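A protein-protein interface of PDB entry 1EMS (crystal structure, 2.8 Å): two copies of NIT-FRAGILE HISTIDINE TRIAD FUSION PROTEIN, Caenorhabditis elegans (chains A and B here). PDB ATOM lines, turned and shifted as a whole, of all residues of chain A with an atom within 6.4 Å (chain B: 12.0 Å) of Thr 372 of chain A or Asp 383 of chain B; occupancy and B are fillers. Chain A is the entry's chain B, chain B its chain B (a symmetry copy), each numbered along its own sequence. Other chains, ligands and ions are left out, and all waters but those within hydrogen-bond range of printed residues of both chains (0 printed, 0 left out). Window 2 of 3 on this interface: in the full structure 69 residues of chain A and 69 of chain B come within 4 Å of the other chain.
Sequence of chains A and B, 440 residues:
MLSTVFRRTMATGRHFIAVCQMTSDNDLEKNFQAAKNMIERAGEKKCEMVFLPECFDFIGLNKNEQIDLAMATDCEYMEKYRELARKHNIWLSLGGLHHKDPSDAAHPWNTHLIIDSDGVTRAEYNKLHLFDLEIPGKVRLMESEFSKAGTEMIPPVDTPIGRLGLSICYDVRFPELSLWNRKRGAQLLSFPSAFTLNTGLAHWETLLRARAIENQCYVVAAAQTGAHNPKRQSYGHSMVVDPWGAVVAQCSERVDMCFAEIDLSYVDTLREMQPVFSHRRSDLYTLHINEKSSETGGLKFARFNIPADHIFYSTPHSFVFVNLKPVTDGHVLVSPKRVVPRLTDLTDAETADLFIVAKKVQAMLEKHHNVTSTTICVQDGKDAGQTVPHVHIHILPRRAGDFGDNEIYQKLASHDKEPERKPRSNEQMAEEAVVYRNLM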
ATOM      1  N   GLU A 366      15.626  10.421 -17.533  1.00  0.00           N
ATOM      2  CA  GLU A 366      16.021  10.496 -16.132  1.00  0.00           C
ATOM      3  C   GLU A 366      17.431  11.035 -15.924  1.00  0.00           C
ATOM      4  O   GLU A 366      17.720  11.656 -14.902  1.00  0.00           O
ATOM      5  CB  GLU A 366      15.891   9.122 -15.485  1.00  0.00           C
ATOM      6  CG  GLU A 366      14.459   8.738 -15.177  1.00  0.00           C
ATOM      7  CD  GLU A 366      14.355   7.349 -14.594  1.00  0.00           C
ATOM      8  OE1 GLU A 366      15.329   6.910 -13.941  1.00  0.00           O
ATOM      9  OE2 GLU A 366      13.300   6.704 -14.780  1.00  0.00           O
ATOM     10  N   ASN A 370      17.091  14.567 -14.524  1.00  0.00           N
ATOM     11  CA  ASN A 370      17.644  14.057 -13.276  1.00  0.00           C
ATOM     12  C   ASN A 370      16.603  13.690 -12.229  1.00  0.00           C
ATOM     13  O   ASN A 370      16.343  14.452 -11.299  1.00  0.00           O
ATOM     14  CB  ASN A 370      18.636  15.059 -12.686  1.00  0.00           C
ATOM     15  CG  ASN A 370      19.998  14.438 -12.433  1.00  0.00           C
ATOM     16  OD1 ASN A 370      20.634  13.908 -13.350  1.00  0.00           O
ATOM     17  ND2 ASN A 370      20.452  14.494 -11.185  1.00  0.00           N
ATOM     18  N   VAL A 371      16.004  12.515 -12.401  1.00  0.00           N
ATOM     19  CA  VAL A 371      15.000  11.995 -11.479  1.00  0.00           C
ATOM     20  C   VAL A 371      15.190  10.483 -11.418  1.00  0.00           C
ATOM     21  O   VAL A 371      16.082   9.943 -12.073  1.00  0.00           O
ATOM     22  CB  VAL A 371      13.563  12.316 -11.947  1.00  0.00           C
ATOM     23  CG1 VAL A 371      13.342  13.818 -11.943  1.00  0.00           C
ATOM     24  CG2 VAL A 371      13.322  11.750 -13.333  1.00  0.00           C
ATOM     25  N   THR A 372      14.364   9.796 -10.637  1.00  0.00           N
ATOM     26  CA  THR A 372      14.490   8.347 -10.508  1.00  0.00           C
ATOM     27  C   THR A 372      13.150   7.625 -10.569  1.00  0.00           C
ATOM     28  O   THR A 372      12.987   6.553  -9.990  1.00  0.00           O
ATOM     29  CB  THR A 372      15.175   7.974  -9.186  1.00  0.00           C
ATOM     30  OG1 THR A 372      14.413   8.506  -8.094  1.00  0.00           O
ATOM     31  CG2 THR A 372      16.583   8.541  -9.137  1.00  0.00           C
ATOM     32  N   SER A 373      12.189   8.208 -11.273  1.00  0.00           N
ATOM     33  CA  SER A 373      10.881   7.587 -11.385  1.00  0.00           C
ATOM     34  C   SER A 373      10.229   7.947 -12.705  1.00  0.00           C
ATOM     35  O   SER A 373      10.386   9.063 -13.200  1.00  0.00           O
ATOM     36  CB  SER A 373       9.979   8.032 -10.228  1.00  0.00           C
ATOM     37  OG  SER A 373      10.504   7.619  -8.978  1.00  0.00           O
ATOM     38  N   THR A 374       9.509   6.988 -13.275  1.00  0.00           N
ATOM     39  CA  THR A 374       8.813   7.199 -14.533  1.00  0.00           C
ATOM     40  C   THR A 374       7.570   6.326 -14.561  1.00  0.00           C
ATOM     41  O   THR A 374       7.530   5.265 -13.937  1.00  0.00           O
ATOM     42  CB  THR A 374       9.702   6.843 -15.741  1.00  0.00           C
ATOM     43  OG1 THR A 374      10.952   7.539 -15.643  1.00  0.00           O
ATOM     44  CG2 THR A 374       9.010   7.244 -17.036  1.00  0.00           C
ATOM     45  N   THR A 375       6.551   6.789 -15.272  1.00  0.00           N
ATOM     46  CA  THR A 375       5.305   6.047 -15.398  1.00  0.00           C
ATOM     47  C   THR A 375       5.060   5.800 -16.878  1.00  0.00           C
ATOM     48  O   THR A 375       5.185   6.711 -17.697  1.00  0.00           O
ATOM     49  CB  THR A 375       4.096   6.839 -14.820  1.00  0.00           C
ATOM     50  OG1 THR A 375       4.297   7.080 -13.421  1.00  0.00           O
ATOM     51  CG2 THR A 375       2.793   6.055 -15.017  1.00  0.00           C
ATOM     52  N   ARG A 398       8.927  11.265 -13.270  1.00  0.00           N
ATOM     53  CA  ARG A 398       8.305  11.759 -12.054  1.00  0.00           C
ATOM     54  C   ARG A 398       9.229  12.340 -10.993  1.00  0.00           C
ATOM     55  O   ARG A 398      10.418  12.012 -10.930  1.00  0.00           O
ATOM     56  CB  ARG A 398       7.474  10.647 -11.427  1.00  0.00           C
ATOM     57  CG  ARG A 398       6.188  10.371 -12.156  1.00  0.00           C
ATOM     58  CD  ARG A 398       5.167   9.914 -11.152  1.00  0.00           C
ATOM     59  NE  ARG A 398       3.802   9.982 -11.657  1.00  0.00           N
ATOM     60  CZ  ARG A 398       2.724   9.810 -10.896  1.00  0.00           C
ATOM     61  NH1 ARG A 398       2.857   9.562  -9.597  1.00  0.00           N
ATOM     62  NH2 ARG A 398       1.512   9.883 -11.431  1.00  0.00           N
ATOM     63  N   ARG A 399       8.648  13.214 -10.167  1.00  0.00           N
ATOM     64  CA  ARG A 399       9.340  13.870  -9.055  1.00  0.00           C
ATOM     65  C   ARG A 399       8.412  13.849  -7.833  1.00  0.00           C
ATOM     66  O   ARG A 399       7.628  12.912  -7.653  1.00  0.00           O
ATOM     67  CB  ARG A 399       9.691  15.332  -9.387  1.00  0.00           C
ATOM     68  CG  ARG A 399      10.451  15.570 -10.690  1.00  0.00           C
ATOM     69  CD  ARG A 399       9.486  15.782 -11.850  1.00  0.00           C
ATOM     70  NE  ARG A 399      10.160  16.221 -13.069  1.00  0.00           N
ATOM     71  CZ  ARG A 399       9.534  16.503 -14.208  1.00  0.00           C
ATOM     72  NH1 ARG A 399       8.213  16.395 -14.293  1.00  0.00           N
ATOM     73  NH2 ARG A 399      10.234  16.887 -15.264  1.00  0.00           N
ATOM     74  N   ALA A 400       8.496  14.895  -7.010  1.00  0.00           N
ATOM     75  CA  ALA A 400       7.675  15.010  -5.803  1.00  0.00           C
ATOM     76  C   ALA A 400       6.312  15.664  -6.071  1.00  0.00           C
ATOM     77  O   ALA A 400       5.280  15.166  -5.609  1.00  0.00           O
ATOM     78  CB  ALA A 400       8.431  15.795  -4.745  1.00  0.00           C
ATOM     79  N   ASP A 402       4.139  16.857  -9.288  1.00  0.00           N
ATOM     80  CA  ASP A 402       3.239  16.189 -10.242  1.00  0.00           C
ATOM     81  C   ASP A 402       1.990  15.536  -9.639  1.00  0.00           C
ATOM     82  O   ASP A 402       1.042  15.197 -10.355  1.00  0.00           O
ATOM     83  CB  ASP A 402       4.016  15.142 -11.061  1.00  0.00           C
ATOM     84  CG  ASP A 402       4.671  14.069 -10.191  1.00  0.00           C
ATOM     85  OD1 ASP A 402       5.601  14.398  -9.419  1.00  0.00           O
ATOM     86  OD2 ASP A 402       4.256  12.889 -10.284  1.00  0.00           O
ATOM     87  N   PRO B 341      13.624  -4.340  -9.948  1.00  0.00           N
ATOM     88  CA  PRO B 341      12.715  -3.221  -9.691  1.00  0.00           C
ATOM     89  C   PRO B 341      12.386  -2.308 -10.874  1.00  0.00           C
ATOM     90  O   PRO B 341      11.221  -1.963 -11.091  1.00  0.00           O
ATOM     91  CB  PRO B 341      13.434  -2.467  -8.583  1.00  0.00           C
ATOM     92  CG  PRO B 341      14.867  -2.601  -9.004  1.00  0.00           C
ATOM     93  CD  PRO B 341      14.960  -4.069  -9.383  1.00  0.00           C
ATOM     94  N   ARG B 342      13.406  -1.924 -11.639  1.00  0.00           N
ATOM     95  CA  ARG B 342      13.212  -1.005 -12.759  1.00  0.00           C
ATOM     96  C   ARG B 342      13.118  -1.619 -14.149  1.00  0.00           C
ATOM     97  O   ARG B 342      13.766  -2.625 -14.436  1.00  0.00           O
ATOM     98  CB  ARG B 342      14.337   0.030 -12.771  1.00  0.00           C
ATOM     99  CG  ARG B 342      14.727   0.558 -11.402  1.00  0.00           C
ATOM    100  CD  ARG B 342      15.232   1.964 -11.538  1.00  0.00           C
ATOM    101  NE  ARG B 342      14.151   2.824 -11.999  1.00  0.00           N
ATOM    102  CZ  ARG B 342      14.310   4.078 -12.407  1.00  0.00           C
ATOM    103  NH1 ARG B 342      15.522   4.625 -12.413  1.00  0.00           N
ATOM    104  NH2 ARG B 342      13.255   4.785 -12.802  1.00  0.00           N
ATOM    105  N   LEU B 343      12.314  -0.987 -15.011  1.00  0.00           N
ATOM    106  CA  LEU B 343      12.138  -1.431 -16.396  1.00  0.00           C
ATOM    107  C   LEU B 343      13.487  -1.293 -17.084  1.00  0.00           C
ATOM    108  O   LEU B 343      13.866  -2.119 -17.915  1.00  0.00           O
ATOM    109  CB  LEU B 343      11.115  -0.558 -17.139  1.00  0.00           C
ATOM    110  CG  LEU B 343       9.610  -0.683 -16.877  1.00  0.00           C
ATOM    111  CD1 LEU B 343       8.892   0.316 -17.769  1.00  0.00           C
ATOM    112  CD2 LEU B 343       9.107  -2.093 -17.165  1.00  0.00           C
ATOM    113  N   THR B 344      14.203  -0.234 -16.725  1.00  0.00           N
ATOM    114  CA  THR B 344      15.517   0.033 -17.284  1.00  0.00           C
ATOM    115  C   THR B 344      16.588  -0.908 -16.729  1.00  0.00           C
ATOM    116  O   THR B 344      17.778  -0.707 -16.974  1.00  0.00           O
ATOM    117  CB  THR B 344      15.947   1.494 -17.025  1.00  0.00           C
ATOM    118  OG1 THR B 344      15.518   1.901 -15.717  1.00  0.00           O
ATOM    119  CG2 THR B 344      15.346   2.419 -18.072  1.00  0.00           C
ATOM    120  N   ASP B 345      16.170  -1.926 -15.977  1.00  0.00           N
ATOM    121  CA  ASP B 345      17.110  -2.905 -15.422  1.00  0.00           C
ATOM    122  C   ASP B 345      16.979  -4.202 -16.205  1.00  0.00           C
ATOM    123  O   ASP B 345      17.809  -5.111 -16.072  1.00  0.00           O
ATOM    124  CB  ASP B 345      16.812  -3.216 -13.950  1.00  0.00           C
ATOM    125  CG  ASP B 345      17.161  -2.078 -13.016  1.00  0.00           C
ATOM    126  OD1 ASP B 345      18.158  -1.362 -13.271  1.00  0.00           O
ATOM    127  OD2 ASP B 345      16.441  -1.919 -12.008  1.00  0.00           O
ATOM    128  N   CYS B 377      -0.244   0.310 -17.220  1.00  0.00           N
ATOM    129  CA  CYS B 377       0.510   1.212 -16.354  1.00  0.00           C
ATOM    130  C   CYS B 377       1.721   0.506 -15.769  1.00  0.00           C
ATOM    131  O   CYS B 377       1.709  -0.711 -15.572  1.00  0.00           O
ATOM    132  CB  CYS B 377      -0.368   1.730 -15.195  1.00  0.00           C
ATOM    133  SG  CYS B 377      -1.128   3.377 -15.415  1.00  0.00           S
ATOM    134  N   VAL B 378       2.768   1.280 -15.509  1.00  0.00           N
ATOM    135  CA  VAL B 378       3.987   0.768 -14.898  1.00  0.00           C
ATOM    136  C   VAL B 378       4.520   1.852 -13.977  1.00  0.00           C
ATOM    137  O   VAL B 378       4.970   2.903 -14.432  1.00  0.00           O
ATOM    138  CB  VAL B 378       5.077   0.422 -15.937  1.00  0.00           C
ATOM    139  CG1 VAL B 378       6.324  -0.099 -15.220  1.00  0.00           C
ATOM    140  CG2 VAL B 378       4.560  -0.627 -16.908  1.00  0.00           C
ATOM    141  N   GLN B 379       4.452   1.596 -12.676  1.00  0.00           N
ATOM    142  CA  GLN B 379       4.926   2.549 -11.684  1.00  0.00           C
ATOM    143  C   GLN B 379       6.384   2.242 -11.378  1.00  0.00           C
ATOM    144  O   GLN B 379       6.696   1.536 -10.424  1.00  0.00           O
ATOM    145  CB  GLN B 379       4.089   2.421 -10.417  1.00  0.00           C
ATOM    146  CG  GLN B 379       2.604   2.415 -10.690  1.00  0.00           C
ATOM    147  CD  GLN B 379       1.803   1.991  -9.484  1.00  0.00           C
ATOM    148  OE1 GLN B 379       1.914   0.855  -9.013  1.00  0.00           O
ATOM    149  NE2 GLN B 379       0.989   2.904  -8.970  1.00  0.00           N
ATOM    150  N   ASP B 380       7.280   2.778 -12.195  1.00  0.00           N
ATOM    151  CA  ASP B 380       8.696   2.529 -12.004  1.00  0.00           C
ATOM    152  C   ASP B 380       9.382   3.613 -11.189  1.00  0.00           C
ATOM    153  O   ASP B 380       9.872   4.600 -11.744  1.00  0.00           O
ATOM    154  CB  ASP B 380       9.387   2.395 -13.356  1.00  0.00           C
ATOM    155  CG  ASP B 380      10.831   2.012 -13.218  1.00  0.00           C
ATOM    156  OD1 ASP B 380      11.618   2.829 -12.698  1.00  0.00           O
ATOM    157  OD2 ASP B 380      11.175   0.884 -13.620  1.00  0.00           O
ATOM    158  N   GLY B 381       9.421   3.416  -9.872  1.00  0.00           N
ATOM    159  CA  GLY B 381      10.049   4.386  -8.990  1.00  0.00           C
ATOM    160  C   GLY B 381       9.172   4.826  -7.828  1.00  0.00           C
ATOM    161  O   GLY B 381       7.943   4.771  -7.903  1.00  0.00           O
ATOM    162  N   LYS B 382       9.808   5.267  -6.746  1.00  0.00           N
ATOM    163  CA  LYS B 382       9.080   5.717  -5.569  1.00  0.00           C
ATOM    164  C   LYS B 382       8.069   6.793  -5.943  1.00  0.00           C
ATOM    165  O   LYS B 382       6.876   6.665  -5.660  1.00  0.00           O
ATOM    166  CB  LYS B 382      10.053   6.277  -4.528  1.00  0.00           C
ATOM    167  CG  LYS B 382      11.090   5.278  -4.031  1.00  0.00           C
ATOM    168  CD  LYS B 382      12.044   5.921  -3.033  1.00  0.00           C
ATOM    169  CE  LYS B 382      11.293   6.508  -1.838  1.00  0.00           C
ATOM    170  NZ  LYS B 382      12.187   7.259  -0.906  1.00  0.00           N
ATOM    171  N   ASP B 383       8.562   7.844  -6.594  1.00  0.00           N
ATOM    172  CA  ASP B 383       7.750   8.985  -7.012  1.00  0.00           C
ATOM    173  C   ASP B 383       6.629   8.634  -7.993  1.00  0.00           C
ATOM    174  O   ASP B 383       5.726   9.440  -8.228  1.00  0.00           O
ATOM    175  CB  ASP B 383       8.661  10.045  -7.632  1.00  0.00           C
ATOM    176  CG  ASP B 383       9.862  10.366  -6.753  1.00  0.00           C
ATOM    177  OD1 ASP B 383       9.670  10.955  -5.668  1.00  0.00           O
ATOM    178  OD2 ASP B 383      11.001  10.019  -7.147  1.00  0.00           O
ATOM    179  N   ALA B 384       6.694   7.434  -8.564  1.00  0.00           N
ATOM    180  CA  ALA B 384       5.691   6.978  -9.523  1.00  0.00           C
ATOM    181  C   ALA B 384       4.631   6.106  -8.858  1.00  0.00           C
ATOM    182  O   ALA B 384       3.624   5.761  -9.478  1.00  0.00           O
ATOM    183  CB  ALA B 384       6.361   6.209 -10.652  1.00  0.00           C
ATOM    184  N   GLY B 385       4.877   5.738  -7.604  1.00  0.00           N
ATOM    185  CA  GLY B 385       3.925   4.923  -6.869  1.00  0.00           C
ATOM    186  C   GLY B 385       4.227   3.437  -6.747  1.00  0.00           C
ATOM    187  O   GLY B 385       3.349   2.660  -6.364  1.00  0.00           O
ATOM    188  N   GLN B 386       5.454   3.024  -7.060  1.00  0.00           N
ATOM    189  CA  GLN B 386       5.795   1.611  -6.960  1.00  0.00           C
ATOM    190  C   GLN B 386       5.832   1.201  -5.486  1.00  0.00           C
ATOM    191  O   GLN B 386       6.636   1.714  -4.702  1.00  0.00           O
ATOM    192  CB  GLN B 386       7.142   1.330  -7.642  1.00  0.00           C
ATOM    193  CG  GLN B 386       7.401  -0.156  -7.887  1.00  0.00           C
ATOM    194  CD  GLN B 386       8.580  -0.415  -8.804  1.00  0.00           C
ATOM    195  OE1 GLN B 386       9.698   0.032  -8.542  1.00  0.00           O
ATOM    196  NE2 GLN B 386       8.334  -1.150  -9.890  1.00  0.00           N
ATOM    197  N   THR B 387       4.951   0.274  -5.122  1.00  0.00           N
ATOM    198  CA  THR B 387       4.840  -0.202  -3.748  1.00  0.00           C
ATOM    199  C   THR B 387       5.664  -1.461  -3.470  1.00  0.00           C
ATOM    200  O   THR B 387       5.715  -1.936  -2.331  1.00  0.00           O
ATOM    201  CB  THR B 387       3.374  -0.501  -3.404  1.00  0.00           C
ATOM    202  OG1 THR B 387       2.951  -1.677  -4.105  1.00  0.00           O
ATOM    203  CG2 THR B 387       2.485   0.659  -3.830  1.00  0.00           C
ATOM    204  N   VAL B 388       6.300  -1.998  -4.511  1.00  0.00           N
ATOM    205  CA  VAL B 388       7.128  -3.202  -4.392  1.00  0.00           C
ATOM    206  C   VAL B 388       8.283  -3.170  -5.408  1.00  0.00           C
ATOM    207  O   VAL B 388       8.068  -2.952  -6.598  1.00  0.00           O
ATOM    208  CB  VAL B 388       6.264  -4.480  -4.590  1.00  0.00           C
ATOM    209  CG1 VAL B 388       5.335  -4.300  -5.776  1.00  0.00           C
ATOM    210  CG2 VAL B 388       7.158  -5.695  -4.791  1.00  0.00           C
ATOM    211  N   PRO B 389       9.525  -3.401  -4.942  1.00  0.00           N
ATOM    212  CA  PRO B 389      10.744  -3.401  -5.763  1.00  0.00           C
ATOM    213  C   PRO B 389      10.857  -4.561  -6.751  1.00  0.00           C
ATOM    214  O   PRO B 389      11.807  -5.347  -6.697  1.00  0.00           O
ATOM    215  CB  PRO B 389      11.848  -3.439  -4.717  1.00  0.00           C
ATOM    216  CG  PRO B 389      11.263  -4.363  -3.707  1.00  0.00           C
ATOM    217  CD  PRO B 389       9.836  -3.842  -3.570  1.00  0.00           C
ATOM    218  N   HIS B 390       9.893  -4.654  -7.658  1.00  0.00           N
ATOM    219  CA  HIS B 390       9.882  -5.717  -8.649  1.00  0.00           C
ATOM    220  C   HIS B 390       8.949  -5.295  -9.773  1.00  0.00           C
ATOM    221  O   HIS B 390       7.731  -5.239  -9.591  1.00  0.00           O
ATOM    222  CB  HIS B 390       9.396  -7.017  -7.998  1.00  0.00           C
ATOM    223  CG  HIS B 390       9.642  -8.242  -8.821  1.00  0.00           C
ATOM    224  ND1 HIS B 390       8.944  -8.520  -9.977  1.00  0.00           N
ATOM    225  CD2 HIS B 390      10.503  -9.271  -8.646  1.00  0.00           C
ATOM    226  CE1 HIS B 390       9.363  -9.668 -10.477  1.00  0.00           C
ATOM    227  NE2 HIS B 390      10.310 -10.145  -9.688  1.00  0.00           N
ATOM    228  N   VAL B 391       9.535  -4.980 -10.924  1.00  0.00           N
ATOM    229  CA  VAL B 391       8.788  -4.553 -12.104  1.00  0.00           C
ATOM    230  C   VAL B 391       7.505  -5.351 -12.331  1.00  0.00           C
ATOM    231  O   VAL B 391       7.529  -6.577 -12.391  1.00  0.00           O
ATOM    232  CB  VAL B 391       9.656  -4.683 -13.381  1.00  0.00           C
ATOM    233  CG1 VAL B 391       8.845  -4.302 -14.604  1.00  0.00           C
ATOM    234  CG2 VAL B 391      10.885  -3.805 -13.270  1.00  0.00           C
ATOM    235  N   HIS B 392       6.381  -4.656 -12.450  1.00  0.00           N
ATOM    236  CA  HIS B 392       5.115  -5.324 -12.717  1.00  0.00           C
ATOM    237  C   HIS B 392       4.236  -4.426 -13.571  1.00  0.00           C
ATOM    238  O   HIS B 392       4.118  -3.230 -13.307  1.00  0.00           O
ATOM    239  CB  HIS B 392       4.391  -5.702 -11.418  1.00  0.00           C
ATOM    240  CG  HIS B 392       4.323  -4.599 -10.412  1.00  0.00           C
ATOM    241  ND1 HIS B 392       3.168  -4.296  -9.724  1.00  0.00           N
ATOM    242  CD2 HIS B 392       5.270  -3.746  -9.954  1.00  0.00           C
ATOM    243  CE1 HIS B 392       3.407  -3.302  -8.886  1.00  0.00           C
ATOM    244  NE2 HIS B 392       4.675  -2.950  -9.006  1.00  0.00           N
ATOM    245  N   HIS B 394       0.711  -3.200 -14.889  1.00  0.00           N
ATOM    246  CA  HIS B 394      -0.689  -3.148 -14.515  1.00  0.00           C
ATOM    247  C   HIS B 394      -1.476  -3.245 -15.808  1.00  0.00           C
ATOM    248  O   HIS B 394      -1.394  -2.362 -16.665  1.00  0.00           O
ATOM    249  CB  HIS B 394      -1.017  -1.826 -13.801  1.00  0.00           C
ATOM    250  CG  HIS B 394      -0.458  -1.725 -12.412  1.00  0.00           C
ATOM    251  ND1 HIS B 394      -0.853  -2.557 -11.386  1.00  0.00           N
ATOM    252  CD2 HIS B 394       0.474  -0.893 -11.884  1.00  0.00           C
ATOM    253  CE1 HIS B 394      -0.189  -2.244 -10.286  1.00  0.00           C
ATOM    254  NE2 HIS B 394       0.622  -1.237 -10.561  1.00  0.00           N
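The backbone carbonyl oxygen (O) of Asp 380 of chain B lies within hydrogen-bond range of the backbone NH (N) of Thr 374 of chain A, 2.9 Å away. The backbone carbonyl oxygen (O) of Arg 399 of chain A sits close to the side-chain carboxylate (OD1) of Asp 383 of chain B (3.5 Å). The guanidinium group (NH2) of Arg 342 of chain B is in hydrogen-bond range of the backbone carbonyl oxygen (O) of Thr 372 of chain A. OG of Ser 373 of chain A sits at hydrogen-bond distance from OD2 of Asp 383 of chain B (3.1 Å). The side-chain carboxylate (OE1) of Glu 366 of chain A lies within salt-bridge range of the guanidinium group (NH1) of Arg 342 of chain B (2.8 Å). The guanidinium group (NH1) of Arg 398 of chain A sits close to the backbone carbonyl oxygen (O) of Asp 383 of chain B (3.2 Å). The side-chain hydroxyl of Ser 373 of chain A sits at hydrogen-bond distance from the backbone NH of Lys 382 of chain B (3.3 Å).
The backbone NH (N) of Leu 343 of chain B lies within hydrogen-bond range of the side-chain carboxylate (OD2) of Asp 380 of chain B (2.6 Å). OG1 of Thr 375 of chain A lies within hydrogen-bond range of NE of Arg 398 of chain A (3.4 Å). N of Gln 386 of chain B lies within hydrogen-bond range of O of Gly 381 of chain B (3.2 Å). O of Glu 366 of chain A is in hydrogen-bond range of N of Val 371 of chain A, at 3.2 Å. The guanidinium group of Arg 342 of chain B is in salt-bridge range of the side-chain carboxylate of Asp 380 of chain B. The side-chain carboxylate (OE2) of Glu 366 of chain A lies within hydrogen-bond range of the side-chain hydroxyl (OG1) of Thr 374 of chain A (2.6 Å).
Among the printed residues, pairs that only touch across the chains: Ser 373 of chain A with Asp 380 of chain B, Ser 373 of chain A with Gly 381 of chain B, Thr 375 of chain A with Val 378 of chain B, Arg 398 of chain A with Ala 384 of chain B, Thr 374 of chain A with Val 378 of chain B, Thr 375 of chain A with Ala 384 of chain B, Thr 374 of chain A with Ala 384 of chain B, Ser 373 of chain A with Ala 384 of chain B, Thr 372 of chain A with Gly 381 of chain B, Thr 372 of chain A with Asp 383 of chain B and Ser 373 of chain A with Arg 342 of chain B.
Glu 366 of chain A touches just one residue of chain B: Arg 342. Of chain B, only Arg 342 (3.3 Å), Gly 381 (3.8 Å) and Asp 383 (3.9 Å) come within 4 Å of Thr 372 of chain A. Thr 374 of chain A touches just these residues of chain B: Val 378, Asp 380 and Ala 384. Printed residues of chain B within 4 Å of Thr 375 of chain A: Val 378 (3.3 Å) and Ala 384 (3.6 Å). Arg 398 of chain A touches just these residues of chain B: Asp 383 and Ala 384. No residue of chain B comes within 4 Å of Ala 400 of chain A. Printed residues of chain A within 4 Å of Arg 342 of chain B: Glu 366, Thr 372 and Ser 373. Of the printed residues of chain A, Asp 383 of chain B touches Thr 372 (3.9 Å), Ser 373 (3.1 Å), Arg 398 (3.0 Å) and Arg 399 (3.0 Å). The nearest residue of chain B that does not touch Thr 372 of chain A is Asp 380 of chain B (4.1 Å). The nearest residue of chain A that does not touch Asp 383 of chain B is Asp 402 of chain A (4.3 Å).
Of the 11 printed residues of chain A, 7 touch a printed residue of chain B. Printed residues of chain A that touch a printed residue of chain B: Glu 366, Thr 372, Ser 373, Thr 374, Thr 375, Arg 398 and Arg 399. Of the 22 printed residues of chain B, 7 touch a printed residue of chain A. Printed residues of chain B that touch a printed residue of chain A: Arg 342, Val 378, Asp 380, Gly 381, Lys 382, Asp 383 and Ala 384. Along chain B the printed residues that touch a printed residue of chain A span positions 342 to 384.
No position is printed for both chains.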
